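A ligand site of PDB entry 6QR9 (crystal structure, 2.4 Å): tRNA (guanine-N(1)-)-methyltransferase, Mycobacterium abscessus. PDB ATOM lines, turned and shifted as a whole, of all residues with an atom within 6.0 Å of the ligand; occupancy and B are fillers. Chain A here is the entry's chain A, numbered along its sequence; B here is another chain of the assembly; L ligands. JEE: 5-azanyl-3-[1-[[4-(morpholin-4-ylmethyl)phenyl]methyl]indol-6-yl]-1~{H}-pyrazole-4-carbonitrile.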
ATOM      1  N   PRO A  59      -1.789 -20.302   4.953  1.00  0.00           N
ATOM      2  CA  PRO A  59      -1.753 -18.960   5.554  1.00  0.00           C
ATOM      3  C   PRO A  59      -1.350 -19.066   7.007  1.00  0.00           C
ATOM      4  O   PRO A  59      -1.493 -20.133   7.619  1.00  0.00           O
ATOM      5  CB  PRO A  59      -3.196 -18.473   5.406  1.00  0.00           C
ATOM      6  CG  PRO A  59      -3.999 -19.723   5.456  1.00  0.00           C
ATOM      7  CD  PRO A  59      -3.164 -20.790   4.791  1.00  0.00           C
ATOM      8  N   VAL A  84      -4.844 -28.383  26.062  1.00  0.00           N
ATOM      9  CA  VAL A  84      -4.522 -27.599  24.889  1.00  0.00           C
ATOM     10  C   VAL A  84      -5.778 -27.133  24.170  1.00  0.00           C
ATOM     11  O   VAL A  84      -6.323 -27.880  23.354  1.00  0.00           O
ATOM     12  CB  VAL A  84      -3.698 -28.389  23.861  1.00  0.00           C
ATOM     13  CG1 VAL A  84      -3.200 -27.441  22.734  1.00  0.00           C
ATOM     14  CG2 VAL A  84      -2.541 -29.137  24.543  1.00  0.00           C
ATOM     15  N   PRO A  85      -6.220 -25.893  24.463  1.00  0.00           N
ATOM     16  CA  PRO A  85      -7.343 -25.323  23.745  1.00  0.00           C
ATOM     17  C   PRO A  85      -7.036 -25.358  22.268  1.00  0.00           C
ATOM     18  O   PRO A  85      -5.910 -25.100  21.862  1.00  0.00           O
ATOM     19  CB  PRO A  85      -7.411 -23.869  24.237  1.00  0.00           C
ATOM     20  CG  PRO A  85      -6.638 -23.880  25.537  1.00  0.00           C
ATOM     21  CD  PRO A  85      -5.583 -24.933  25.375  1.00  0.00           C
ATOM     22  N   THR A  86      -8.039 -25.656  21.470  1.00  0.00           N
ATOM     23  CA  THR A  86      -7.873 -25.739  20.034  1.00  0.00           C
ATOM     24  C   THR A  86      -9.209 -25.777  19.350  1.00  0.00           C
ATOM     25  O   THR A  86     -10.149 -26.472  19.811  1.00  0.00           O
ATOM     26  CB  THR A  86      -7.036 -26.973  19.623  1.00  0.00           C
ATOM     27  OG1 THR A  86      -7.116 -27.150  18.204  1.00  0.00           O
ATOM     28  CG2 THR A  86      -7.508 -28.219  20.344  1.00  0.00           C
ATOM     29  N   PRO A  87      -9.313 -25.044  18.240  1.00  0.00           N
ATOM     30  CA  PRO A  87     -10.557 -25.012  17.467  1.00  0.00           C
ATOM     31  C   PRO A  87     -10.860 -26.359  16.807  1.00  0.00           C
ATOM     32  O   PRO A  87     -11.923 -26.511  16.209  1.00  0.00           O
ATOM     33  CB  PRO A  87     -10.291 -23.906  16.425  1.00  0.00           C
ATOM     34  CG  PRO A  87      -8.831 -23.945  16.230  1.00  0.00           C
ATOM     35  CD  PRO A  87      -8.226 -24.309  17.575  1.00  0.00           C
ATOM     36  N   CYS A 110      -1.616 -22.239  25.782  1.00  0.00           N
ATOM     37  CA  CYS A 110      -2.339 -21.311  24.909  1.00  0.00           C
ATOM     38  C   CYS A 110      -1.543 -20.935  23.663  1.00  0.00           C
ATOM     39  O   CYS A 110      -0.536 -20.210  23.745  1.00  0.00           O
ATOM     40  CB  CYS A 110      -2.712 -20.037  25.678  1.00  0.00           C
ATOM     41  SG  CYS A 110      -3.612 -20.364  27.201  1.00  0.00           S
ATOM     42  N   GLY A 111      -2.004 -21.415  22.518  1.00  0.00           N
ATOM     43  CA  GLY A 111      -1.363 -21.081  21.269  1.00  0.00           C
ATOM     44  C   GLY A 111      -1.912 -19.818  20.625  1.00  0.00           C
ATOM     45  O   GLY A 111      -2.884 -19.210  21.092  1.00  0.00           O
ATOM     46  N   ARG A 112      -1.255 -19.413  19.554  1.00  0.00           N
ATOM     47  CA  ARG A 112      -1.696 -18.270  18.779  1.00  0.00           C
ATOM     48  C   ARG A 112      -1.456 -18.584  17.323  1.00  0.00           C
ATOM     49  O   ARG A 112      -1.010 -19.697  16.999  1.00  0.00           O
ATOM     50  CB  ARG A 112      -0.954 -17.012  19.212  1.00  0.00           C
ATOM     51  CG  ARG A 112      -1.451 -16.488  20.524  1.00  0.00           C
ATOM     52  CD  ARG A 112      -2.396 -15.339  20.280  1.00  0.00           C
ATOM     53  NE  ARG A 112      -3.430 -15.281  21.293  1.00  0.00           N
ATOM     54  CZ  ARG A 112      -4.337 -14.316  21.384  1.00  0.00           C
ATOM     55  NH1 ARG A 112      -4.352 -13.301  20.512  1.00  0.00           N
ATOM     56  NH2 ARG A 112      -5.248 -14.368  22.339  1.00  0.00           N
ATOM     57  N   TYR A 113      -1.723 -17.622  16.450  1.00  0.00           N
ATOM     58  CA  TYR A 113      -1.548 -17.853  15.013  1.00  0.00           C
ATOM     59  C   TYR A 113      -2.385 -19.065  14.597  1.00  0.00           C
ATOM     60  O   TYR A 113      -3.504 -19.229  15.057  1.00  0.00           O
ATOM     61  CB  TYR A 113      -0.064 -18.060  14.657  1.00  0.00           C
ATOM     62  CG  TYR A 113       0.878 -17.023  15.220  1.00  0.00           C
ATOM     63  CD1 TYR A 113       1.467 -17.192  16.465  1.00  0.00           C
ATOM     64  CD2 TYR A 113       1.203 -15.881  14.508  1.00  0.00           C
ATOM     65  CE1 TYR A 113       2.333 -16.244  16.987  1.00  0.00           C
ATOM     66  CE2 TYR A 113       2.074 -14.934  15.017  1.00  0.00           C
ATOM     67  CZ  TYR A 113       2.633 -15.126  16.258  1.00  0.00           C
ATOM     68  OH  TYR A 113       3.511 -14.185  16.777  1.00  0.00           O
ATOM     69  N   GLU A 114      -1.821 -19.937  13.769  1.00  0.00           N
ATOM     70  CA  GLU A 114      -2.540 -21.158  13.352  1.00  0.00           C
ATOM     71  C   GLU A 114      -2.417 -22.291  14.356  1.00  0.00           C
ATOM     72  O   GLU A 114      -2.936 -23.383  14.130  1.00  0.00           O
ATOM     73  CB  GLU A 114      -2.038 -21.641  11.995  1.00  0.00           C
ATOM     74  CG  GLU A 114      -2.094 -20.557  10.933  1.00  0.00           C
ATOM     75  CD  GLU A 114      -3.483 -19.939  10.817  1.00  0.00           C
ATOM     76  OE1 GLU A 114      -3.680 -18.789  11.300  1.00  0.00           O
ATOM     77  OE2 GLU A 114      -4.374 -20.606  10.265  1.00  0.00           O
ATOM     78  N   GLY A 115      -1.718 -22.022  15.465  1.00  0.00           N
ATOM     79  CA  GLY A 115      -1.570 -22.996  16.521  1.00  0.00           C
ATOM     80  C   GLY A 115      -0.160 -23.532  16.710  1.00  0.00           C
ATOM     81  O   GLY A 115       0.828 -22.963  16.254  1.00  0.00           O
ATOM     82  N   ILE A 116      -0.087 -24.650  17.410  1.00  0.00           N
ATOM     83  CA  ILE A 116       1.167 -25.240  17.860  1.00  0.00           C
ATOM     84  C   ILE A 116       1.522 -26.468  17.016  1.00  0.00           C
ATOM     85  O   ILE A 116       0.645 -27.260  16.704  1.00  0.00           O
ATOM     86  CB  ILE A 116       1.041 -25.643  19.345  1.00  0.00           C
ATOM     87  CG1 ILE A 116       0.605 -24.440  20.182  1.00  0.00           C
ATOM     88  CG2 ILE A 116       2.321 -26.250  19.872  1.00  0.00           C
ATOM     89  CD1 ILE A 116       0.480 -24.757  21.680  1.00  0.00           C
ATOM     90  N   VAL A 133      -9.027 -29.690  23.413  1.00  0.00           N
ATOM     91  CA  VAL A 133     -10.437 -29.365  23.605  1.00  0.00           C
ATOM     92  C   VAL A 133     -10.814 -28.038  22.977  1.00  0.00           C
ATOM     93  O   VAL A 133      -9.980 -27.136  22.864  1.00  0.00           O
ATOM     94  CB  VAL A 133     -10.797 -29.317  25.106  1.00  0.00           C
ATOM     95  CG1 VAL A 133     -10.631 -30.717  25.741  1.00  0.00           C
ATOM     96  CG2 VAL A 133      -9.942 -28.263  25.818  1.00  0.00           C
ATOM     97  N   SER A 134     -12.080 -27.921  22.571  1.00  0.00           N
ATOM     98  CA  SER A 134     -12.646 -26.636  22.147  1.00  0.00           C
ATOM     99  C   SER A 134     -13.804 -26.240  23.039  1.00  0.00           C
ATOM    100  O   SER A 134     -14.595 -27.101  23.439  1.00  0.00           O
ATOM    101  CB  SER A 134     -13.128 -26.711  20.706  1.00  0.00           C
ATOM    102  OG  SER A 134     -14.012 -25.645  20.456  1.00  0.00           O
ATOM    103  N   ILE A 135     -13.903 -24.958  23.351  1.00  0.00           N
ATOM    104  CA  ILE A 135     -14.946 -24.499  24.269  1.00  0.00           C
ATOM    105  C   ILE A 135     -16.254 -24.147  23.593  1.00  0.00           C
ATOM    106  O   ILE A 135     -17.228 -23.807  24.283  1.00  0.00           O
ATOM    107  CB  ILE A 135     -14.515 -23.275  25.092  1.00  0.00           C
ATOM    108  CG1 ILE A 135     -14.273 -22.066  24.190  1.00  0.00           C
ATOM    109  CG2 ILE A 135     -13.319 -23.595  25.982  1.00  0.00           C
ATOM    110  CD1 ILE A 135     -14.157 -20.757  24.987  1.00  0.00           C
ATOM    111  N   GLY A 136     -16.322 -24.227  22.274  1.00  0.00           N
ATOM    112  CA  GLY A 136     -17.560 -23.908  21.588  1.00  0.00           C
ATOM    113  C   GLY A 136     -17.363 -23.744  20.089  1.00  0.00           C
ATOM    114  O   GLY A 136     -16.234 -23.608  19.634  1.00  0.00           O
ATOM    115  N   ASP A 137     -18.464 -23.747  19.339  1.00  0.00           N
ATOM    116  CA  ASP A 137     -18.406 -23.706  17.891  1.00  0.00           C
ATOM    117  C   ASP A 137     -18.280 -22.292  17.333  1.00  0.00           C
ATOM    118  O   ASP A 137     -19.210 -21.787  16.709  1.00  0.00           O
ATOM    119  CB  ASP A 137     -19.641 -24.389  17.288  1.00  0.00           C
ATOM    120  CG  ASP A 137     -19.568 -25.913  17.379  1.00  0.00           C
ATOM    121  OD1 ASP A 137     -18.473 -26.491  17.183  1.00  0.00           O
ATOM    122  OD2 ASP A 137     -20.612 -26.526  17.673  1.00  0.00           O
ATOM    123  N   TYR A 138     -17.126 -21.676  17.554  1.00  0.00           N
ATOM    124  CA  TYR A 138     -16.836 -20.367  16.998  1.00  0.00           C
ATOM    125  C   TYR A 138     -15.328 -20.256  16.968  1.00  0.00           C
ATOM    126  O   TYR A 138     -14.643 -21.084  17.554  1.00  0.00           O
ATOM    127  CB  TYR A 138     -17.457 -19.243  17.830  1.00  0.00           C
ATOM    128  CG  TYR A 138     -17.443 -19.563  19.296  1.00  0.00           C
ATOM    129  CD1 TYR A 138     -16.256 -19.571  20.018  1.00  0.00           C
ATOM    130  CD2 TYR A 138     -18.627 -19.891  19.962  1.00  0.00           C
ATOM    131  CE1 TYR A 138     -16.247 -19.888  21.384  1.00  0.00           C
ATOM    132  CE2 TYR A 138     -18.621 -20.201  21.334  1.00  0.00           C
ATOM    133  CZ  TYR A 138     -17.425 -20.196  22.029  1.00  0.00           C
ATOM    134  OH  TYR A 138     -17.406 -20.513  23.368  1.00  0.00           O
ATOM    135  N   VAL A 139     -14.814 -19.234  16.283  1.00  0.00           N
ATOM    136  CA  VAL A 139     -13.373 -19.073  16.137  1.00  0.00           C
ATOM    137  C   VAL A 139     -12.869 -17.889  16.943  1.00  0.00           C
ATOM    138  O   VAL A 139     -13.410 -16.796  16.856  1.00  0.00           O
ATOM    139  CB  VAL A 139     -12.984 -18.873  14.633  1.00  0.00           C
ATOM    140  CG1 VAL A 139     -11.483 -18.681  14.493  1.00  0.00           C
ATOM    141  CG2 VAL A 139     -13.459 -20.044  13.777  1.00  0.00           C
ATOM    142  N   LEU A 140     -11.826 -18.136  17.715  1.00  0.00           N
ATOM    143  CA  LEU A 140     -11.131 -17.128  18.520  1.00  0.00           C
ATOM    144  C   LEU A 140      -9.747 -16.795  17.920  1.00  0.00           C
ATOM    145  O   LEU A 140      -9.370 -17.329  16.880  1.00  0.00           O
ATOM    146  CB  LEU A 140     -11.004 -17.643  19.941  1.00  0.00           C
ATOM    147  CG  LEU A 140     -12.366 -17.994  20.572  1.00  0.00           C
ATOM    148  CD1 LEU A 140     -12.212 -18.769  21.844  1.00  0.00           C
ATOM    149  CD2 LEU A 140     -13.241 -16.725  20.818  1.00  0.00           C
ATOM    150  N   ASN A 141      -8.991 -15.911  18.576  1.00  0.00           N
ATOM    151  CA  ASN A 141      -7.671 -15.548  18.088  1.00  0.00           C
ATOM    152  C   ASN A 141      -6.568 -16.431  18.647  1.00  0.00           C
ATOM    153  O   ASN A 141      -5.448 -16.461  18.124  1.00  0.00           O
ATOM    154  CB  ASN A 141      -7.348 -14.105  18.445  1.00  0.00           C
ATOM    155  CG  ASN A 141      -8.200 -13.114  17.681  1.00  0.00           C
ATOM    156  OD1 ASN A 141      -8.379 -13.231  16.466  1.00  0.00           O
ATOM    157  ND2 ASN A 141      -8.739 -12.132  18.396  1.00  0.00           N
ATOM    158  N   GLY A 142      -6.885 -17.125  19.737  1.00  0.00           N
ATOM    159  CA  GLY A 142      -5.896 -17.937  20.419  1.00  0.00           C
ATOM    160  C   GLY A 142      -6.567 -18.593  21.596  1.00  0.00           C
ATOM    161  O   GLY A 142      -7.772 -18.417  21.776  1.00  0.00           O
ATOM    162  N   GLY A 143      -5.817 -19.339  22.400  1.00  0.00           N
ATOM    163  CA  GLY A 143      -6.418 -20.132  23.463  1.00  0.00           C
ATOM    164  C   GLY A 143      -6.598 -19.472  24.821  1.00  0.00           C
ATOM    165  O   GLY A 143      -7.093 -20.117  25.746  1.00  0.00           O
ATOM    166  N   ALA A 146     -10.225 -19.189  26.009  1.00  0.00           N
ATOM    167  CA  ALA A 146     -10.645 -20.548  26.284  1.00  0.00           C
ATOM    168  C   ALA A 146     -10.143 -20.965  27.660  1.00  0.00           C
ATOM    169  O   ALA A 146     -10.866 -21.588  28.449  1.00  0.00           O
ATOM    170  CB  ALA A 146     -10.115 -21.509  25.212  1.00  0.00           C
ATOM    171  N   ARG B 156     -13.210  -9.980  15.572  1.00  0.00           N
ATOM    172  CA  ARG B 156     -12.258 -10.452  14.583  1.00  0.00           C
ATOM    173  C   ARG B 156     -12.884 -10.601  13.197  1.00  0.00           C
ATOM    174  O   ARG B 156     -12.174 -10.814  12.219  1.00  0.00           O
ATOM    175  CB  ARG B 156     -11.606 -11.761  15.039  1.00  0.00           C
ATOM    176  CG  ARG B 156     -12.573 -12.929  15.178  1.00  0.00           C
ATOM    177  CD  ARG B 156     -11.863 -14.138  15.782  1.00  0.00           C
ATOM    178  NE  ARG B 156     -10.762 -14.598  14.938  1.00  0.00           N
ATOM    179  CZ  ARG B 156     -10.945 -15.306  13.824  1.00  0.00           C
ATOM    180  NH1 ARG B 156     -12.171 -15.619  13.434  1.00  0.00           N
ATOM    181  NH2 ARG B 156      -9.905 -15.694  13.107  1.00  0.00           N
ATOM    182  N   GLU B 182      -9.982 -28.435  11.480  1.00  0.00           N
ATOM    183  CA  GLU B 182      -8.653 -28.373  10.896  1.00  0.00           C
ATOM    184  C   GLU B 182      -7.746 -29.486  11.381  1.00  0.00           C
ATOM    185  O   GLU B 182      -7.833 -29.928  12.534  1.00  0.00           O
ATOM    186  CB  GLU B 182      -7.996 -27.019  11.167  1.00  0.00           C
ATOM    187  CG  GLU B 182      -8.626 -25.855  10.413  1.00  0.00           C
ATOM    188  CD  GLU B 182      -8.522 -26.000   8.895  1.00  0.00           C
ATOM    189  OE1 GLU B 182      -8.979 -27.018   8.313  1.00  0.00           O
ATOM    190  OE2 GLU B 182      -7.938 -25.099   8.268  1.00  0.00           O
HETATM  191  C10 JEE L   1      -6.663 -22.211  20.421  1.00  0.00           C
HETATM  192  C13 JEE L   1      -4.702 -20.363  17.867  1.00  0.00           C
HETATM  193  C15 JEE L   1      -6.449 -19.326  16.481  1.00  0.00           C
HETATM  194  C17 JEE L   1      -6.045 -21.091  14.680  1.00  0.00           C
HETATM  195  C20 JEE L   1      -8.055 -22.141  11.556  1.00  0.00           C
HETATM  196  C22 JEE L   1      -7.454 -20.305  10.364  1.00  0.00           C
HETATM  197  C26 JEE L   1      -8.691 -22.042   9.430  1.00  0.00           C
HETATM  198  C28 JEE L   1      -8.036 -19.718  14.582  1.00  0.00           C
HETATM  199  N01 JEE L   1     -13.700 -22.753  20.536  1.00  0.00           N
HETATM  200  C02 JEE L   1     -12.511 -22.186  19.995  1.00  0.00           C
HETATM  201  N03 JEE L   1     -12.449 -21.309  18.966  1.00  0.00           N
HETATM  202  N04 JEE L   1     -11.157 -21.009  18.740  1.00  0.00           N
HETATM  203  C05 JEE L   1     -10.378 -21.630  19.619  1.00  0.00           C
HETATM  204  C06 JEE L   1      -8.850 -21.561  19.598  1.00  0.00           C
HETATM  205  C07 JEE L   1      -8.239 -20.845  18.548  1.00  0.00           C
HETATM  206  C08 JEE L   1      -6.816 -20.775  18.465  1.00  0.00           C
HETATM  207  C09 JEE L   1      -6.040 -21.452  19.390  1.00  0.00           C
HETATM  208  C11 JEE L   1      -8.070 -22.273  20.517  1.00  0.00           C
HETATM  209  C12 JEE L   1      -4.674 -21.183  18.996  1.00  0.00           C
HETATM  210  N14 JEE L   1      -5.979 -20.151  17.568  1.00  0.00           N
HETATM  211  C16 JEE L   1      -6.855 -20.091  15.227  1.00  0.00           C
HETATM  212  C18 JEE L   1      -6.442 -21.753  13.502  1.00  0.00           C
HETATM  213  C19 JEE L   1      -7.632 -21.395  12.854  1.00  0.00           C
HETATM  214  N21 JEE L   1      -8.325 -21.360  10.573  1.00  0.00           N
HETATM  215  C23 JEE L   1      -7.139 -19.950   8.920  1.00  0.00           C
HETATM  216  O24 JEE L   1      -6.863 -21.045   8.127  1.00  0.00           O
HETATM  217  C25 JEE L   1      -7.537 -22.200   8.455  1.00  0.00           C
HETATM  218  C27 JEE L   1      -8.428 -20.380  13.421  1.00  0.00           C
HETATM  219  C29 JEE L   1     -11.201 -22.406  20.412  1.00  0.00           C
HETATM  220  C30 JEE L   1     -10.803 -23.331  21.565  1.00  0.00           C
HETATM  221  N31 JEE L   1     -10.526 -24.017  22.428  1.00  0.00           N
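The backbone NH of Val 133 sits at hydrogen-bond distance from the backbone carbonyl oxygen of Val 84, at 3.3 Å. The side-chain sulfur (SG) of Cys 110 sits at hydrogen-bond distance from the backbone carbonyl oxygen (O) of Gly 143, at 3.8 Å. O of Gly 136 is in hydrogen-bond range of OG of Ser 134 (3.1 Å). O of Gly 111 lies within hydrogen-bond range of N of Gly 143 (3.2 Å). The backbone carbonyl oxygen (O) of Val 133 sits at hydrogen-bond distance from the backbone NH (N) of Thr 86 (2.8 Å). O of Ile 135 is in hydrogen-bond range of OH of Tyr 138. The side-chain amide oxygen (OD1) of Asn 141 sits at hydrogen-bond distance from the guanidinium group (NE) of Arg 156 of chain B (3.1 Å).
N04 of the ligand lies within hydrogen-bond range of N of Leu 140, 3.1 Å away. The backbone NH (N) of Thr 86 sits at hydrogen-bond distance from a nitrogen (N31) of the ligand (3.1 Å). N01 of the ligand sits at hydrogen-bond distance from OG of Ser 134 (2.9 Å). The backbone carbonyl oxygen of Gly 136 is in hydrogen-bond range of a nitrogen (N01) of the ligand (2.8 Å). O of Tyr 138 lies within hydrogen-bond range of N03 of the ligand (2.6 Å).
The side-chain carboxylate of Glu 114 lies close to an oxygen (O24) of the ligand (3.3 Å). The backbone carbonyl oxygen of Val 133 lies close to a nitrogen (N31) of the ligand, 3.2 Å away. O of Pro 85 touches C10 of the ligand (3.3 Å). Pro 87 touches the ligand (CD to C06, 3.5 Å). Gly 111 touches the ligand. C of Arg 112 touches C13 of the ligand, at 3.7 Å. Tyr 113 touches the ligand. Ile 135 touches the ligand (N to N01, 3.6 Å). CG1 of Val 139 touches C28 of the ligand, at 3.6 Å. O of Asn 141 touches C15 of the ligand, 3.5 Å away. CA of Gly 142 touches C08 of the ligand, at 3.6 Å. N of Gly 143 touches C10 of the ligand, at 3.6 Å. Ala 146 touches the ligand (CB to N31, 3.8 Å). Glu 182 of chain B touches the ligand (OE2 to C25, 2.9 Å). 19 residues have an atom within 4 Å of the ligand: Pro 85, Thr 86, Pro 87, Gly 111, Arg 112, Tyr 113, Glu 114, Val 133, Ser 134, Ile 135, Gly 136, Tyr 138, Val 139, Leu 140, Asn 141, Gly 142, Gly 143, Ala 146 and Glu 182 of chain B. Along chain A the residues within 4 Å of the ligand span positions 85 to 146.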
